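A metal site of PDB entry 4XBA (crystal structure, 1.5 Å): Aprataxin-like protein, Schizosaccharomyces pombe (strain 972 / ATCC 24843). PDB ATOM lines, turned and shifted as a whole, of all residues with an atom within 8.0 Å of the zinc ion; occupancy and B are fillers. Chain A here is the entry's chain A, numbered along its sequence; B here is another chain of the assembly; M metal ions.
The side-chain sulfur (SG) of Cys 168 sits close to the backbone NH (N) of Arg 170, at 3.3 Å. SG of Cys 171 lies close to N of Glu 173. NH1 of Arg 170 lies within salt-bridge range of OE1 of Glu 189 (2.7 Å). The backbone carbonyl oxygen (O) of Glu 173 sits at hydrogen-bond distance from the backbone NH (N) of Cys 168 (2.8 Å).
The zinc ion is bound by NE2 of His 185 (2.0 Å), OE2 of Glu 189 (2.1 Å), SG of Cys 171 (2.2 Å) and SG of Cys 168 (2.3 Å).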
ATOM      1  N   TYR A 134     -15.087 -15.230   9.884  1.00  0.00           N
ATOM      2  CA  TYR A 134     -15.816 -15.768  11.042  1.00  0.00           C
ATOM      3  C   TYR A 134     -14.867 -16.415  12.070  1.00  0.00           C
ATOM      4  O   TYR A 134     -14.948 -16.123  13.271  1.00  0.00           O
ATOM      5  CB  TYR A 134     -16.874 -16.764  10.555  1.00  0.00           C
ATOM      6  CG  TYR A 134     -17.626 -17.426  11.668  1.00  0.00           C
ATOM      7  CD1 TYR A 134     -18.588 -16.681  12.392  1.00  0.00           C
ATOM      8  CD2 TYR A 134     -17.403 -18.738  11.968  1.00  0.00           C
ATOM      9  CE1 TYR A 134     -19.320 -17.294  13.471  1.00  0.00           C
ATOM     10  CE2 TYR A 134     -18.134 -19.356  13.010  1.00  0.00           C
ATOM     11  CZ  TYR A 134     -19.081 -18.635  13.706  1.00  0.00           C
ATOM     12  OH  TYR A 134     -19.770 -19.296  14.694  1.00  0.00           O
ATOM     13  N   LYS A 167     -18.452 -24.059  12.997  1.00  0.00           N
ATOM     14  CA  LYS A 167     -19.193 -24.278  14.216  1.00  0.00           C
ATOM     15  C   LYS A 167     -19.864 -23.020  14.734  1.00  0.00           C
ATOM     16  O   LYS A 167     -19.224 -21.973  14.771  1.00  0.00           O
ATOM     17  CB  LYS A 167     -18.220 -24.796  15.273  1.00  0.00           C
ATOM     18  CG  LYS A 167     -18.802 -25.160  16.610  1.00  0.00           C
ATOM     19  CD  LYS A 167     -17.680 -25.808  17.458  1.00  0.00           C
ATOM     20  CE  LYS A 167     -18.159 -26.338  18.806  1.00  0.00           C
ATOM     21  NZ  LYS A 167     -18.575 -27.780  18.713  1.00  0.00           N
ATOM     22  N   CYS A 168     -21.138 -23.135  15.091  1.00  0.00           N
ATOM     23  CA  CYS A 168     -21.864 -22.029  15.739  1.00  0.00           C
ATOM     24  C   CYS A 168     -21.219 -21.708  17.084  1.00  0.00           C
ATOM     25  O   CYS A 168     -21.097 -22.576  17.939  1.00  0.00           O
ATOM     26  CB  CYS A 168     -23.354 -22.374  15.943  1.00  0.00           C
ATOM     27  SG  CYS A 168     -24.184 -21.077  16.855  1.00  0.00           S
ATOM     28  N   TRP A 169     -20.878 -20.453  17.284  1.00  0.00           N
ATOM     29  CA  TRP A 169     -20.198 -20.040  18.513  1.00  0.00           C
ATOM     30  C   TRP A 169     -21.119 -20.174  19.710  1.00  0.00           C
ATOM     31  O   TRP A 169     -20.621 -20.308  20.848  1.00  0.00           O
ATOM     32  CB  TRP A 169     -19.708 -18.566  18.448  1.00  0.00           C
ATOM     33  CG  TRP A 169     -20.809 -17.576  18.304  1.00  0.00           C
ATOM     34  CD1 TRP A 169     -21.320 -17.089  17.127  1.00  0.00           C
ATOM     35  CD2 TRP A 169     -21.564 -16.985  19.347  1.00  0.00           C
ATOM     36  NE1 TRP A 169     -22.333 -16.209  17.401  1.00  0.00           N
ATOM     37  CE2 TRP A 169     -22.522 -16.150  18.760  1.00  0.00           C
ATOM     38  CE3 TRP A 169     -21.540 -17.104  20.725  1.00  0.00           C
ATOM     39  CZ2 TRP A 169     -23.441 -15.444  19.496  1.00  0.00           C
ATOM     40  CZ3 TRP A 169     -22.410 -16.349  21.474  1.00  0.00           C
ATOM     41  CH2 TRP A 169     -23.383 -15.542  20.860  1.00  0.00           C
ATOM     42  N   ARG A 170     -22.453 -20.132  19.537  1.00  0.00           N
ATOM     43  CA  ARG A 170     -23.405 -20.044  20.642  1.00  0.00           C
ATOM     44  C   ARG A 170     -23.850 -21.426  21.087  1.00  0.00           C
ATOM     45  O   ARG A 170     -23.953 -21.665  22.320  1.00  0.00           O
ATOM     46  CB  ARG A 170     -24.625 -19.177  20.275  1.00  0.00           C
ATOM     47  CG  ARG A 170     -25.584 -18.820  21.428  1.00  0.00           C
ATOM     48  CD  ARG A 170     -26.536 -17.660  21.031  1.00  0.00           C
ATOM     49  NE  ARG A 170     -27.340 -17.198  22.174  1.00  0.00           N
ATOM     50  CZ  ARG A 170     -28.655 -17.369  22.291  1.00  0.00           C
ATOM     51  NH1 ARG A 170     -29.335 -17.983  21.317  1.00  0.00           N
ATOM     52  NH2 ARG A 170     -29.299 -16.918  23.382  1.00  0.00           N
ATOM     53  N   CYS A 171     -24.146 -22.324  20.155  1.00  0.00           N
ATOM     54  CA  CYS A 171     -24.661 -23.661  20.526  1.00  0.00           C
ATOM     55  C   CYS A 171     -23.790 -24.841  20.126  1.00  0.00           C
ATOM     56  O   CYS A 171     -24.059 -25.977  20.549  1.00  0.00           O
ATOM     57  CB  CYS A 171     -26.054 -23.910  19.981  1.00  0.00           C
ATOM     58  SG  CYS A 171     -26.064 -24.242  18.150  1.00  0.00           S
ATOM     59  N   GLY A 172     -22.796 -24.602  19.298  1.00  0.00           N
ATOM     60  CA  GLY A 172     -21.882 -25.664  18.932  1.00  0.00           C
ATOM     61  C   GLY A 172     -22.315 -26.534  17.754  1.00  0.00           C
ATOM     62  O   GLY A 172     -21.602 -27.452  17.403  1.00  0.00           O
ATOM     63  N   GLU A 173     -23.478 -26.296  17.163  1.00  0.00           N
ATOM     64  CA  GLU A 173     -23.853 -27.011  15.951  1.00  0.00           C
ATOM     65  C   GLU A 173     -22.841 -26.773  14.838  1.00  0.00           C
ATOM     66  O   GLU A 173     -22.288 -25.680  14.721  1.00  0.00           O
ATOM     67  CB  GLU A 173     -25.233 -26.570  15.472  1.00  0.00           C
ATOM     68  CG  GLU A 173     -25.734 -27.354  14.284  1.00  0.00           C
ATOM     69  CD  GLU A 173     -27.178 -27.052  13.919  1.00  0.00           C
ATOM     70  OE1 GLU A 173     -27.878 -26.398  14.726  1.00  0.00           O
ATOM     71  OE2 GLU A 173     -27.578 -27.420  12.779  1.00  0.00           O
ATOM     72  N   THR A 174     -22.603 -27.800  14.032  1.00  0.00           N
ATOM     73  CA  THR A 174     -21.635 -27.665  12.942  1.00  0.00           C
ATOM     74  C   THR A 174     -22.240 -27.833  11.586  1.00  0.00           C
ATOM     75  O   THR A 174     -23.313 -28.406  11.406  1.00  0.00           O
ATOM     76  CB  THR A 174     -20.472 -28.635  13.087  1.00  0.00           C
ATOM     77  OG1 THR A 174     -20.948 -29.980  13.077  1.00  0.00           O
ATOM     78  CG2 THR A 174     -19.702 -28.346  14.395  1.00  0.00           C
ATOM     79  N   PHE A 175     -21.546 -27.236  10.612  1.00  0.00           N
ATOM     80  CA  PHE A 175     -22.085 -26.995   9.293  1.00  0.00           C
ATOM     81  C   PHE A 175     -21.157 -27.407   8.170  1.00  0.00           C
ATOM     82  O   PHE A 175     -21.417 -27.074   7.011  1.00  0.00           O
ATOM     83  CB  PHE A 175     -22.412 -25.503   9.153  1.00  0.00           C
ATOM     84  CG  PHE A 175     -23.488 -25.084  10.083  1.00  0.00           C
ATOM     85  CD1 PHE A 175     -23.223 -24.767  11.380  1.00  0.00           C
ATOM     86  CD2 PHE A 175     -24.779 -25.190   9.691  1.00  0.00           C
ATOM     87  CE1 PHE A 175     -24.259 -24.500  12.276  1.00  0.00           C
ATOM     88  CE2 PHE A 175     -25.814 -24.880  10.538  1.00  0.00           C
ATOM     89  CZ  PHE A 175     -25.554 -24.562  11.860  1.00  0.00           C
ATOM     90  N   LEU A 182     -24.370 -21.850   7.776  1.00  0.00           N
ATOM     91  CA  LEU A 182     -23.979 -21.270   9.039  1.00  0.00           C
ATOM     92  C   LEU A 182     -24.533 -19.848   9.210  1.00  0.00           C
ATOM     93  O   LEU A 182     -25.057 -19.503  10.270  1.00  0.00           O
ATOM     94  CB  LEU A 182     -22.455 -21.267   9.214  1.00  0.00           C
ATOM     95  CG  LEU A 182     -22.006 -20.498  10.459  1.00  0.00           C
ATOM     96  CD1 LEU A 182     -22.459 -21.171  11.744  1.00  0.00           C
ATOM     97  CD2 LEU A 182     -20.478 -20.363  10.410  1.00  0.00           C
ATOM     98  N   HIS A 185     -28.105 -19.891  10.190  1.00  0.00           N
ATOM     99  CA  HIS A 185     -28.221 -20.268  11.591  1.00  0.00           C
ATOM    100  C   HIS A 185     -27.803 -19.139  12.528  1.00  0.00           C
ATOM    101  O   HIS A 185     -28.437 -18.953  13.584  1.00  0.00           O
ATOM    102  CB  HIS A 185     -27.369 -21.515  11.843  1.00  0.00           C
ATOM    103  CG  HIS A 185     -27.356 -21.949  13.273  1.00  0.00           C
ATOM    104  ND1 HIS A 185     -28.298 -22.815  13.788  1.00  0.00           N
ATOM    105  CD2 HIS A 185     -26.455 -21.730  14.243  1.00  0.00           C
ATOM    106  CE1 HIS A 185     -28.007 -23.032  15.075  1.00  0.00           C
ATOM    107  NE2 HIS A 185     -26.917 -22.361  15.376  1.00  0.00           N
ATOM    108  N   LEU A 186     -26.738 -18.389  12.188  1.00  0.00           N
ATOM    109  CA  LEU A 186     -26.365 -17.238  13.042  1.00  0.00           C
ATOM    110  C   LEU A 186     -27.509 -16.224  13.108  1.00  0.00           C
ATOM    111  O   LEU A 186     -27.760 -15.626  14.146  1.00  0.00           O
ATOM    112  CB  LEU A 186     -25.068 -16.578  12.543  1.00  0.00           C
ATOM    113  CG  LEU A 186     -23.799 -17.406  12.621  1.00  0.00           C
ATOM    114  CD1 LEU A 186     -22.664 -16.757  11.838  1.00  0.00           C
ATOM    115  CD2 LEU A 186     -23.383 -17.621  14.053  1.00  0.00           C
ATOM    116  N   GLU A 188     -30.728 -16.958  12.984  1.00  0.00           N
ATOM    117  CA  GLU A 188     -31.679 -17.542  13.915  1.00  0.00           C
ATOM    118  C   GLU A 188     -31.207 -17.368  15.355  1.00  0.00           C
ATOM    119  O   GLU A 188     -32.010 -17.116  16.254  1.00  0.00           O
ATOM    120  CB  GLU A 188     -31.851 -19.040  13.612  1.00  0.00           C
ATOM    121  CG  GLU A 188     -32.464 -19.329  12.243  1.00  0.00           C
ATOM    122  CD  GLU A 188     -33.908 -18.933  12.134  1.00  0.00           C
ATOM    123  OE1 GLU A 188     -34.562 -18.750  13.182  1.00  0.00           O
ATOM    124  OE2 GLU A 188     -34.391 -18.813  10.988  1.00  0.00           O
ATOM    125  N   GLU A 189     -29.908 -17.498  15.598  1.00  0.00           N
ATOM    126  CA  GLU A 189     -29.392 -17.387  16.973  1.00  0.00           C
ATOM    127  C   GLU A 189     -29.541 -15.972  17.466  1.00  0.00           C
ATOM    128  O   GLU A 189     -29.718 -15.722  18.683  1.00  0.00           O
ATOM    129  CB  GLU A 189     -27.904 -17.781  17.044  1.00  0.00           C
ATOM    130  CG  GLU A 189     -27.647 -19.275  16.926  1.00  0.00           C
ATOM    131  CD  GLU A 189     -27.945 -20.019  18.252  1.00  0.00           C
ATOM    132  OE1 GLU A 189     -28.605 -19.485  19.153  1.00  0.00           O
ATOM    133  OE2 GLU A 189     -27.509 -21.179  18.361  1.00  0.00           O
ATOM    134  N   TYR A 190     -29.312 -15.010  16.553  1.00  0.00           N
ATOM    135  CA  TYR A 190     -29.453 -13.626  16.907  1.00  0.00           C
ATOM    136  C   TYR A 190     -30.926 -13.315  17.223  1.00  0.00           C
ATOM    137  O   TYR A 190     -31.238 -12.629  18.211  1.00  0.00           O
ATOM    138  CB  TYR A 190     -28.938 -12.724  15.782  1.00  0.00           C
ATOM    139  CG  TYR A 190     -29.216 -11.261  16.028  1.00  0.00           C
ATOM    140  CD1 TYR A 190     -28.605 -10.570  17.055  1.00  0.00           C
ATOM    141  CD2 TYR A 190     -30.130 -10.599  15.259  1.00  0.00           C
ATOM    142  CE1 TYR A 190     -28.867  -9.255  17.296  1.00  0.00           C
ATOM    143  CE2 TYR A 190     -30.390  -9.266  15.457  1.00  0.00           C
ATOM    144  CZ  TYR A 190     -29.769  -8.588  16.500  1.00  0.00           C
ATOM    145  OH  TYR A 190     -30.030  -7.250  16.735  1.00  0.00           O
ATOM    146  N   PRO B 148     -21.659 -24.222  25.227  1.00  0.00           N
ATOM    147  CA  PRO B 148     -22.381 -25.044  24.227  1.00  0.00           C
ATOM    148  C   PRO B 148     -22.512 -26.536  24.600  1.00  0.00           C
ATOM    149  O   PRO B 148     -21.568 -27.085  25.120  1.00  0.00           O
ATOM    150  CB  PRO B 148     -21.529 -24.875  22.966  1.00  0.00           C
ATOM    151  CG  PRO B 148     -20.789 -23.595  23.149  1.00  0.00           C
ATOM    152  CD  PRO B 148     -20.543 -23.462  24.650  1.00  0.00           C
HETATM  153 ZN    ZN M   1     -26.180 -22.229  17.181  1.00  0.00          ZN
